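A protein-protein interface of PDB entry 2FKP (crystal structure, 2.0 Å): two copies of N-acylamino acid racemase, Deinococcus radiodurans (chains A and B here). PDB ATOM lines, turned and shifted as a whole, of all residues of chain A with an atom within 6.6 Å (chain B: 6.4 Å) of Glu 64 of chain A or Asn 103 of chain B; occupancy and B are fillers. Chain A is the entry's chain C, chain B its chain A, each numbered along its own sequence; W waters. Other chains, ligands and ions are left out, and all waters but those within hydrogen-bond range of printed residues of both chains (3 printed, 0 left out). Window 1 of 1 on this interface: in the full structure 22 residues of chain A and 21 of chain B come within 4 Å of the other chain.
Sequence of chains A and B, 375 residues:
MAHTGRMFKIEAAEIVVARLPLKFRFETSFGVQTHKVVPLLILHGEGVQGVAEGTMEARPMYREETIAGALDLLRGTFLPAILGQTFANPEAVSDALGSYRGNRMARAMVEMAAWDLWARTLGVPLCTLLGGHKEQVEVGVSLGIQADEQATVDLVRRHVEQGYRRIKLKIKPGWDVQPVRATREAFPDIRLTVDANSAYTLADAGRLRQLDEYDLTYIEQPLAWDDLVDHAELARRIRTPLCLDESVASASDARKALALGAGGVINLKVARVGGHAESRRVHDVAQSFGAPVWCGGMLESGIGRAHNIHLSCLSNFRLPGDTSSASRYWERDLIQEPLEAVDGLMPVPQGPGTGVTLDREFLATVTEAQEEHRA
The backbone carbonyl oxygen of Arg 101 of chain B lies close to the side-chain amide oxygen of Asn 103 of chain B. The side-chain carboxylate (OE1) of Glu 57 of chain A lies within hydrogen-bond range of the backbone NH (N) of Met 61 of chain A (3.1 Å). The backbone carbonyl oxygen (O) of Leu 73 of chain B lies within hydrogen-bond range of the backbone NH (N) of Phe 78 of chain B, at 3.0 Å. The guanidinium group of Arg 63 of chain A is in salt-bridge range of the side-chain carboxylate of Glu 64 of chain A (2.9 Å). The side-chain carboxylate of Glu 57 of chain A sits at hydrogen-bond distance from the backbone NH of Tyr 62 of chain A.
Arg 59 of chain A touches Tyr 100 of chain B. Pro 60 of chain A touches Leu 73 of chain B (CD to CD1, 3.6 Å). Pro 60 of chain A touches Tyr 100 of chain B. OD1 of Asn 103 of chain B touches CB of Pro 60 of chain A, at 3.4 Å. Met 61 of chain A touches Tyr 100 of chain B. O of Met 61 of chain A touches CD of Arg 101 of chain B, at 3.3 Å. CA of Glu 64 of chain A touches O of Arg 101 of chain B, at 3.9 Å. Trp 225 of chain A touches Arg 101 of chain B (CD1 to NE, 3.6 Å). N of Gly 102 of chain B touches CZ2 of Trp 225 of chain A, 3.8 Å away.
Asn 103 of chain B touches just these residues of chain A: Pro 60 (3.4 Å) and Glu 64 (3.0 Å). Printed residues of chain A within 4 Å of Gly 102 of chain B: Trp 225. Of the printed residues of chain B, Met 61 of chain A touches Tyr 100 and Arg 101. Of the printed residues of chain A, Leu 73 of chain B touches Pro 60. Of the printed residues of chain B, Trp 225 of chain A touches Arg 101 and Gly 102. Ala 108 of chain B touches none of the printed residues of chain A. Met 105 of chain B touches none of the printed residues of chain A. The nearest residue of chain B that does not touch Glu 64 of chain A is Gly 102 of chain B (4.3 Å).
The side-chain amide oxygen (OD1) of Asn 103 of chain B sits close to the backbone carbonyl oxygen (O) of Glu 64 of chain A. NH1 of Arg 101 of chain B sits at hydrogen-bond distance from O of Tyr 62 of chain A, at 2.7 Å. The side-chain amide nitrogen (ND2) of Asn 103 of chain A sits at hydrogen-bond distance from the backbone carbonyl oxygen (O) of Glu 64 of chain B (2.8 Å). The backbone NH (N) of Arg 101 of chain B sits at hydrogen-bond distance from the backbone carbonyl oxygen (O) of Pro 60 of chain A, 2.8 Å away.
Of the 14 printed residues of chain A, 7 touch a printed residue of chain B. Hydrophobic or aromatic side chains of chain A within 4 Å of the printed part of chain B: Pro 60, Met 61 and Trp 225. Hydrophobic or aromatic side chains of chain B within 4 Å of the printed part of chain A: Leu 73 and Tyr 100. Along chain B the printed residues that touch a printed residue of chain A span positions 64 to 103.
Glu 64 of chain A touches Asn 103 of chain B, and with the chains exchanged Asn 103 of chain A touches Glu 64 of chain B. 6 positions are printed for both chains.
Water W1 lies within hydrogen-bond range of the backbone carbonyl oxygen of Gly 69 of chain B (2.7 Å), the side-chain hydroxyl of Thr 66 of chain A (2.8 Å) and the backbone NH of Leu 73 of chain B (3.5 Å). Water W3 lies within hydrogen-bond range of ND2 of Asn 103 of chain B (3.0 Å) and O of Glu 64 of chain A (3.0 Å). Water W2 lies within hydrogen-bond range of the backbone carbonyl oxygen of Glu 64 of chain B (3.0 Å) and the side-chain amide oxygen of Asn 103 of chain A (3.1 Å).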
ATOM      1  N   GLU A  57       9.686  19.964  -3.419  1.00  0.00           N
ATOM      2  CA  GLU A  57       8.333  19.588  -3.032  1.00  0.00           C
ATOM      3  C   GLU A  57       7.634  20.750  -2.368  1.00  0.00           C
ATOM      4  O   GLU A  57       8.276  21.713  -1.944  1.00  0.00           O
ATOM      5  CB  GLU A  57       8.399  18.419  -2.044  1.00  0.00           C
ATOM      6  CG  GLU A  57       9.485  17.391  -2.396  1.00  0.00           C
ATOM      7  CD  GLU A  57       9.914  16.553  -1.207  1.00  0.00           C
ATOM      8  OE1 GLU A  57      10.779  16.990  -0.412  1.00  0.00           O
ATOM      9  OE2 GLU A  57       9.400  15.417  -1.100  1.00  0.00           O
ATOM     10  N   ARG A  59       6.493  20.639   0.564  1.00  0.00           N
ATOM     11  CA  ARG A  59       7.067  20.602   1.905  1.00  0.00           C
ATOM     12  C   ARG A  59       8.428  19.944   1.869  1.00  0.00           C
ATOM     13  O   ARG A  59       8.670  19.068   1.040  1.00  0.00           O
ATOM     14  CB  ARG A  59       6.139  19.879   2.889  1.00  0.00           C
ATOM     15  CG  ARG A  59       4.828  20.618   3.081  1.00  0.00           C
ATOM     16  CD  ARG A  59       3.892  19.940   4.062  1.00  0.00           C
ATOM     17  NE  ARG A  59       2.759  20.823   4.318  1.00  0.00           N
ATOM     18  CZ  ARG A  59       1.759  21.022   3.454  1.00  0.00           C
ATOM     19  NH1 ARG A  59       1.748  20.384   2.276  1.00  0.00           N
ATOM     20  NH2 ARG A  59       0.765  21.858   3.756  1.00  0.00           N
ATOM     21  N   PRO A  60       9.322  20.355   2.780  1.00  0.00           N
ATOM     22  CA  PRO A  60      10.701  19.843   2.820  1.00  0.00           C
ATOM     23  C   PRO A  60      10.789  18.459   3.492  1.00  0.00           C
ATOM     24  O   PRO A  60      11.091  18.345   4.687  1.00  0.00           O
ATOM     25  CB  PRO A  60      11.438  20.902   3.632  1.00  0.00           C
ATOM     26  CG  PRO A  60      10.356  21.457   4.557  1.00  0.00           C
ATOM     27  CD  PRO A  60       9.050  21.343   3.846  1.00  0.00           C
ATOM     28  N   MET A  61      10.538  17.421   2.699  1.00  0.00           N
ATOM     29  CA  MET A  61      10.464  16.057   3.198  1.00  0.00           C
ATOM     30  C   MET A  61      11.659  15.224   2.700  1.00  0.00           C
ATOM     31  O   MET A  61      12.339  14.549   3.483  1.00  0.00           O
ATOM     32  CB  MET A  61       9.127  15.439   2.779  1.00  0.00           C
ATOM     33  CG  MET A  61       7.889  16.086   3.455  1.00  0.00           C
ATOM     34  SD  MET A  61       6.353  15.540   2.637  1.00  0.00           S
ATOM     35  CE  MET A  61       6.697  15.976   0.940  1.00  0.00           C
ATOM     36  N   TYR A  62      11.951  15.300   1.411  1.00  0.00           N
ATOM     37  CA  TYR A  62      13.158  14.652   0.894  1.00  0.00           C
ATOM     38  C   TYR A  62      14.420  15.487   1.168  1.00  0.00           C
ATOM     39  O   TYR A  62      15.479  14.952   1.523  1.00  0.00           O
ATOM     40  CB  TYR A  62      13.047  14.352  -0.611  1.00  0.00           C
ATOM     41  CG  TYR A  62      14.397  14.119  -1.252  1.00  0.00           C
ATOM     42  CD1 TYR A  62      15.030  15.130  -1.955  1.00  0.00           C
ATOM     43  CD2 TYR A  62      15.052  12.893  -1.130  1.00  0.00           C
ATOM     44  CE1 TYR A  62      16.283  14.934  -2.541  1.00  0.00           C
ATOM     45  CE2 TYR A  62      16.321  12.683  -1.716  1.00  0.00           C
ATOM     46  CZ  TYR A  62      16.914  13.722  -2.414  1.00  0.00           C
ATOM     47  OH  TYR A  62      18.133  13.583  -3.000  1.00  0.00           O
ATOM     48  N   ARG A  63      14.324  16.789   0.951  1.00  0.00           N
ATOM     49  CA  ARG A  63      15.422  17.692   1.306  1.00  0.00           C
ATOM     50  C   ARG A  63      14.838  19.042   1.670  1.00  0.00           C
ATOM     51  O   ARG A  63      13.630  19.146   1.962  1.00  0.00           O
ATOM     52  CB  ARG A  63      16.484  17.792   0.186  1.00  0.00           C
ATOM     53  CG  ARG A  63      17.927  17.650   0.652  1.00  0.00           C
ATOM     54  CD  ARG A  63      18.912  17.689  -0.542  1.00  0.00           C
ATOM     55  NE  ARG A  63      20.326  17.529  -0.179  1.00  0.00           N
ATOM     56  CZ  ARG A  63      21.110  18.501   0.303  1.00  0.00           C
ATOM     57  NH1 ARG A  63      20.620  19.717   0.513  1.00  0.00           N
ATOM     58  NH2 ARG A  63      22.388  18.257   0.608  1.00  0.00           N
ATOM     59  N   GLU A  64      15.665  20.076   1.608  1.00  0.00           N
ATOM     60  CA  GLU A  64      15.369  21.347   2.287  1.00  0.00           C
ATOM     61  C   GLU A  64      14.582  22.395   1.489  1.00  0.00           C
ATOM     62  O   GLU A  64      13.991  23.291   2.085  1.00  0.00           O
ATOM     63  CB  GLU A  64      16.665  21.954   2.857  1.00  0.00           C
ATOM     64  CG  GLU A  64      17.448  22.870   1.889  1.00  0.00           C
ATOM     65  CD  GLU A  64      18.161  22.141   0.745  1.00  0.00           C
ATOM     66  OE1 GLU A  64      18.841  22.822  -0.045  1.00  0.00           O
ATOM     67  OE2 GLU A  64      18.028  20.915   0.593  1.00  0.00           O
ATOM     68  N   GLU A  65      14.541  22.284   0.157  1.00  0.00           N
ATOM     69  CA  GLU A  65      13.812  23.285  -0.635  1.00  0.00           C
ATOM     70  C   GLU A  65      12.305  23.032  -0.710  1.00  0.00           C
ATOM     71  O   GLU A  65      11.822  21.920  -0.519  1.00  0.00           O
ATOM     72  CB  GLU A  65      14.398  23.418  -2.054  1.00  0.00           C
ATOM     73  CG  GLU A  65      15.905  23.845  -2.057  1.00  0.00           C
ATOM     74  CD  GLU A  65      16.489  23.791  -3.447  1.00  0.00           C
ATOM     75  OE1 GLU A  65      16.105  24.644  -4.289  1.00  0.00           O
ATOM     76  OE2 GLU A  65      17.308  22.884  -3.711  1.00  0.00           O
ATOM     77  N   THR A  66      11.571  24.085  -1.010  1.00  0.00           N
ATOM     78  CA  THR A  66      10.127  23.988  -1.177  1.00  0.00           C
ATOM     79  C   THR A  66       9.736  24.738  -2.421  1.00  0.00           C
ATOM     80  O   THR A  66      10.486  25.609  -2.901  1.00  0.00           O
ATOM     81  CB  THR A  66       9.378  24.624   0.001  1.00  0.00           C
ATOM     82  OG1 THR A  66       9.655  26.026   0.043  1.00  0.00           O
ATOM     83  CG2 THR A  66       9.805  23.980   1.339  1.00  0.00           C
ATOM     84  N   GLY A 102      23.005  27.836  -1.498  1.00  0.00           N
ATOM     85  CA  GLY A 102      22.116  26.689  -1.542  1.00  0.00           C
ATOM     86  C   GLY A 102      21.106  26.807  -2.663  1.00  0.00           C
ATOM     87  O   GLY A 102      21.429  27.282  -3.764  1.00  0.00           O
ATOM     88  N   ASN A 103      19.885  26.367  -2.394  1.00  0.00           N
ATOM     89  CA  ASN A 103      18.831  26.408  -3.397  1.00  0.00           C
ATOM     90  C   ASN A 103      19.259  25.822  -4.747  1.00  0.00           C
ATOM     91  O   ASN A 103      19.017  26.408  -5.798  1.00  0.00           O
ATOM     92  CB  ASN A 103      18.298  27.845  -3.546  1.00  0.00           C
ATOM     93  CG  ASN A 103      17.658  28.356  -2.249  1.00  0.00           C
ATOM     94  OD1 ASN A 103      16.451  28.184  -2.041  1.00  0.00           O
ATOM     95  ND2 ASN A 103      18.476  28.934  -1.347  1.00  0.00           N
ATOM     96  N   ARG A 104      19.888  24.660  -4.715  1.00  0.00           N
ATOM     97  CA  ARG A 104      20.417  24.057  -5.943  1.00  0.00           C
ATOM     98  C   ARG A 104      19.344  23.548  -6.920  1.00  0.00           C
ATOM     99  O   ARG A 104      19.513  23.615  -8.126  1.00  0.00           O
ATOM    100  CB  ARG A 104      21.362  22.921  -5.586  1.00  0.00           C
ATOM    101  CG  ARG A 104      22.549  23.396  -4.789  1.00  0.00           C
ATOM    102  CD  ARG A 104      23.786  22.827  -5.368  1.00  0.00           C
ATOM    103  NE  ARG A 104      24.981  23.422  -4.800  1.00  0.00           N
ATOM    104  CZ  ARG A 104      26.127  23.515  -5.469  1.00  0.00           C
ATOM    105  NH1 ARG A 104      26.185  23.045  -6.714  1.00  0.00           N
ATOM    106  NH2 ARG A 104      27.199  24.084  -4.902  1.00  0.00           N
ATOM    107  N   MET A 105      18.250  23.025  -6.397  1.00  0.00           N
ATOM    108  CA  MET A 105      17.146  22.647  -7.278  1.00  0.00           C
ATOM    109  C   MET A 105      16.466  23.853  -7.965  1.00  0.00           C
ATOM    110  O   MET A 105      16.019  23.723  -9.110  1.00  0.00           O
ATOM    111  CB  MET A 105      16.116  21.800  -6.533  1.00  0.00           C
ATOM    112  CG  MET A 105      16.696  20.515  -5.942  1.00  0.00           C
ATOM    113  SD  MET A 105      15.371  19.582  -5.124  1.00  0.00           S
ATOM    114  CE  MET A 105      16.220  18.162  -4.412  1.00  0.00           C
ATOM    115  N   TRP A 225      20.545  12.507   6.296  1.00  0.00           N
ATOM    116  CA  TRP A 225      20.479  13.005   4.927  1.00  0.00           C
ATOM    117  C   TRP A 225      21.584  13.987   4.612  1.00  0.00           C
ATOM    118  O   TRP A 225      21.971  14.148   3.445  1.00  0.00           O
ATOM    119  CB  TRP A 225      19.120  13.673   4.666  1.00  0.00           C
ATOM    120  CG  TRP A 225      18.914  14.960   5.429  1.00  0.00           C
ATOM    121  CD1 TRP A 225      18.359  15.099   6.677  1.00  0.00           C
ATOM    122  CD2 TRP A 225      19.268  16.290   5.000  1.00  0.00           C
ATOM    123  NE1 TRP A 225      18.344  16.427   7.041  1.00  0.00           N
ATOM    124  CE2 TRP A 225      18.883  17.179   6.031  1.00  0.00           C
ATOM    125  CE3 TRP A 225      19.845  16.814   3.841  1.00  0.00           C
ATOM    126  CZ2 TRP A 225      19.089  18.562   5.945  1.00  0.00           C
ATOM    127  CZ3 TRP A 225      20.045  18.184   3.754  1.00  0.00           C
ATOM    128  CH2 TRP A 225      19.664  19.045   4.794  1.00  0.00           C
ATOM    129  N   GLU B  64      20.764  29.631   3.367  1.00  0.00           N
ATOM    130  CA  GLU B  64      19.942  29.132   2.257  1.00  0.00           C
ATOM    131  C   GLU B  64      18.451  29.485   2.350  1.00  0.00           C
ATOM    132  O   GLU B  64      17.723  29.380   1.350  1.00  0.00           O
ATOM    133  CB  GLU B  64      20.125  27.612   2.112  1.00  0.00           C
ATOM    134  CG  GLU B  64      19.231  26.776   3.028  1.00  0.00           C
ATOM    135  CD  GLU B  64      19.702  26.660   4.496  1.00  0.00           C
ATOM    136  OE1 GLU B  64      19.115  25.801   5.195  1.00  0.00           O
ATOM    137  OE2 GLU B  64      20.610  27.404   4.961  1.00  0.00           O
ATOM    138  N   GLU B  65      17.987  29.867   3.545  1.00  0.00           N
ATOM    139  CA  GLU B  65      16.552  30.080   3.745  1.00  0.00           C
ATOM    140  C   GLU B  65      16.140  31.470   3.272  1.00  0.00           C
ATOM    141  O   GLU B  65      16.970  32.375   3.157  1.00  0.00           O
ATOM    142  CB  GLU B  65      16.152  29.873   5.207  1.00  0.00           C
ATOM    143  CG  GLU B  65      16.285  28.435   5.685  1.00  0.00           C
ATOM    144  CD  GLU B  65      15.948  28.318   7.143  1.00  0.00           C
ATOM    145  OE1 GLU B  65      14.750  28.471   7.524  1.00  0.00           O
ATOM    146  OE2 GLU B  65      16.895  28.127   7.918  1.00  0.00           O
ATOM    147  N   GLY B  69       9.959  31.261   1.594  1.00  0.00           N
ATOM    148  CA  GLY B  69       9.985  29.846   1.958  1.00  0.00           C
ATOM    149  C   GLY B  69       9.570  29.626   3.399  1.00  0.00           C
ATOM    150  O   GLY B  69       8.716  28.749   3.693  1.00  0.00           O
ATOM    151  N   ALA B  70      10.170  30.415   4.305  1.00  0.00           N
ATOM    152  CA  ALA B  70       9.966  30.239   5.739  1.00  0.00           C
ATOM    153  C   ALA B  70       8.519  30.493   6.142  1.00  0.00           C
ATOM    154  O   ALA B  70       7.934  29.723   6.905  1.00  0.00           O
ATOM    155  CB  ALA B  70      10.873  31.170   6.517  1.00  0.00           C
ATOM    156  N   LEU B  73       6.222  27.877   4.970  1.00  0.00           N
ATOM    157  CA  LEU B  73       6.404  26.705   5.817  1.00  0.00           C
ATOM    158  C   LEU B  73       5.681  26.862   7.167  1.00  0.00           C
ATOM    159  O   LEU B  73       5.030  25.931   7.634  1.00  0.00           O
ATOM    160  CB  LEU B  73       7.885  26.393   5.981  1.00  0.00           C
ATOM    161  CG  LEU B  73       8.291  25.143   6.733  1.00  0.00           C
ATOM    162  CD1 LEU B  73       7.727  23.856   6.089  1.00  0.00           C
ATOM    163  CD2 LEU B  73       9.819  25.131   6.789  1.00  0.00           C
ATOM    164  N   PHE B  78       4.021  24.184   9.859  1.00  0.00           N
ATOM    165  CA  PHE B  78       4.373  24.208  11.283  1.00  0.00           C
ATOM    166  C   PHE B  78       3.205  24.661  12.188  1.00  0.00           C
ATOM    167  O   PHE B  78       2.904  24.058  13.214  1.00  0.00           O
ATOM    168  CB  PHE B  78       5.608  25.101  11.523  1.00  0.00           C
ATOM    169  CG  PHE B  78       6.889  24.570  10.923  1.00  0.00           C
ATOM    170  CD1 PHE B  78       6.963  23.278  10.407  1.00  0.00           C
ATOM    171  CD2 PHE B  78       8.040  25.359  10.928  1.00  0.00           C
ATOM    172  CE1 PHE B  78       8.158  22.788   9.880  1.00  0.00           C
ATOM    173  CE2 PHE B  78       9.245  24.892  10.413  1.00  0.00           C
ATOM    174  CZ  PHE B  78       9.308  23.608   9.877  1.00  0.00           C
ATOM    175  N   TYR B 100      10.459  17.279   9.149  1.00  0.00           N
ATOM    176  CA  TYR B 100      10.843  18.096   7.998  1.00  0.00           C
ATOM    177  C   TYR B 100      12.336  18.360   7.987  1.00  0.00           C
ATOM    178  O   TYR B 100      12.967  18.367   9.030  1.00  0.00           O
ATOM    179  CB  TYR B 100       9.993  19.360   7.950  1.00  0.00           C
ATOM    180  CG  TYR B 100       8.527  18.984   7.847  1.00  0.00           C
ATOM    181  CD1 TYR B 100       7.715  18.915   8.989  1.00  0.00           C
ATOM    182  CD2 TYR B 100       7.969  18.649   6.618  1.00  0.00           C
ATOM    183  CE1 TYR B 100       6.383  18.548   8.890  1.00  0.00           C
ATOM    184  CE2 TYR B 100       6.645  18.282   6.511  1.00  0.00           C
ATOM    185  CZ  TYR B 100       5.862  18.233   7.644  1.00  0.00           C
ATOM    186  OH  TYR B 100       4.555  17.853   7.515  1.00  0.00           O
ATOM    187  N   ARG B 101      12.904  18.537   6.800  1.00  0.00           N
ATOM    188  CA  ARG B 101      14.352  18.596   6.667  1.00  0.00           C
ATOM    189  C   ARG B 101      14.827  20.039   6.524  1.00  0.00           C
ATOM    190  O   ARG B 101      14.141  20.870   5.909  1.00  0.00           O
ATOM    191  CB  ARG B 101      14.826  17.710   5.511  1.00  0.00           C
ATOM    192  CG  ARG B 101      14.676  16.209   5.847  1.00  0.00           C
ATOM    193  CD  ARG B 101      15.262  15.275   4.806  1.00  0.00           C
ATOM    194  NE  ARG B 101      15.277  13.895   5.322  1.00  0.00           N
ATOM    195  CZ  ARG B 101      15.475  12.798   4.593  1.00  0.00           C
ATOM    196  NH1 ARG B 101      15.681  12.865   3.272  1.00  0.00           N
ATOM    197  NH2 ARG B 101      15.463  11.619   5.201  1.00  0.00           N
ATOM    198  N   GLY B 102      15.983  20.321   7.122  1.00  0.00           N
ATOM    199  CA  GLY B 102      16.563  21.657   7.108  1.00  0.00           C
ATOM    200  C   GLY B 102      15.647  22.720   7.703  1.00  0.00           C
ATOM    201  O   GLY B 102      14.980  22.502   8.735  1.00  0.00           O
ATOM    202  N   ASN B 103      15.626  23.865   7.033  1.00  0.00           N
ATOM    203  CA  ASN B 103      14.788  25.009   7.408  1.00  0.00           C
ATOM    204  C   ASN B 103      14.906  25.346   8.889  1.00  0.00           C
ATOM    205  O   ASN B 103      13.905  25.505   9.574  1.00  0.00           O
ATOM    206  CB  ASN B 103      13.332  24.791   6.987  1.00  0.00           C
ATOM    207  CG  ASN B 103      13.194  24.563   5.507  1.00  0.00           C
ATOM    208  OD1 ASN B 103      13.323  23.412   5.012  1.00  0.00           O
ATOM    209  ND2 ASN B 103      12.980  25.647   4.769  1.00  0.00           N
ATOM    210  N   ARG B 104      16.142  25.452   9.383  1.00  0.00           N
ATOM    211  CA  ARG B 104      16.347  25.598  10.836  1.00  0.00           C
ATOM    212  C   ARG B 104      15.882  26.931  11.405  1.00  0.00           C
ATOM    213  O   ARG B 104      15.366  26.976  12.530  1.00  0.00           O
ATOM    214  CB  ARG B 104      17.799  25.327  11.215  1.00  0.00           C
ATOM    215  CG  ARG B 104      18.231  23.907  10.854  1.00  0.00           C
ATOM    216  CD  ARG B 104      19.161  23.332  11.874  1.00  0.00           C
ATOM    217  NE  ARG B 104      19.311  21.874  11.773  1.00  0.00           N
ATOM    218  CZ  ARG B 104      19.349  21.050  12.829  1.00  0.00           C
ATOM    219  NH1 ARG B 104      19.208  21.526  14.072  1.00  0.00           N
ATOM    220  NH2 ARG B 104      19.493  19.736  12.646  1.00  0.00           N
ATOM    221  N   MET B 105      16.055  28.004  10.634  1.00  0.00           N
ATOM    222  CA  MET B 105      15.584  29.328  11.049  1.00  0.00           C
ATOM    223  C   MET B 105      14.047  29.434  11.091  1.00  0.00           C
ATOM    224  O   MET B 105      13.499  30.099  11.964  1.00  0.00           O
ATOM    225  CB  MET B 105      16.182  30.427  10.156  1.00  0.00           C
ATOM    226  CG  MET B 105      17.691  30.411  10.105  1.00  0.00           C
ATOM    227  SD  MET B 105      18.276  31.811   9.141  1.00  0.00           S
ATOM    228  CE  MET B 105      20.042  31.633   9.425  1.00  0.00           C
ATOM    229  N   ALA B 106      13.357  28.791  10.144  1.00  0.00           N
ATOM    230  CA  ALA B 106      11.895  28.727  10.204  1.00  0.00           C
ATOM    231  C   ALA B 106      11.490  27.973  11.459  1.00  0.00           C
ATOM    232  O   ALA B 106      10.618  28.404  12.212  1.00  0.00           O
ATOM    233  CB  ALA B 106      11.321  28.041   8.962  1.00  0.00           C
ATOM    234  N   ARG B 107      12.119  26.819  11.670  1.00  0.00           N
ATOM    235  CA  ARG B 107      11.893  26.047  12.868  1.00  0.00           C
ATOM    236  C   ARG B 107      12.159  26.866  14.128  1.00  0.00           C
ATOM    237  O   ARG B 107      11.415  26.782  15.075  1.00  0.00           O
ATOM    238  CB  ARG B 107      12.766  24.794  12.859  1.00  0.00           C
ATOM    239  CG  ARG B 107      12.189  23.705  11.969  1.00  0.00           C
ATOM    240  CD  ARG B 107      13.057  22.506  11.988  1.00  0.00           C
ATOM    241  NE  ARG B 107      12.862  21.856  13.266  1.00  0.00           N
ATOM    242  CZ  ARG B 107      12.251  20.695  13.413  1.00  0.00           C
ATOM    243  NH1 ARG B 107      11.841  20.039  12.332  1.00  0.00           N
ATOM    244  NH2 ARG B 107      12.113  20.182  14.632  1.00  0.00           N
ATOM    245  N   ALA B 108      13.234  27.651  14.124  1.00  0.00           N
ATOM    246  CA  ALA B 108      13.615  28.421  15.307  1.00  0.00           C
ATOM    247  C   ALA B 108      12.554  29.450  15.671  1.00  0.00           C
ATOM    248  O   ALA B 108      12.383  29.779  16.841  1.00  0.00           O
ATOM    249  CB  ALA B 108      14.994  29.090  15.122  1.00  0.00           C
HETATM  250  O   HOH W   1       7.938  26.697   2.161  1.00  0.00           O
HETATM  251  O   HOH W   2      16.372  26.763   0.671  1.00  0.00           O
HETATM  252  O   HOH W   3      15.332  25.894   2.935  1.00  0.00           O
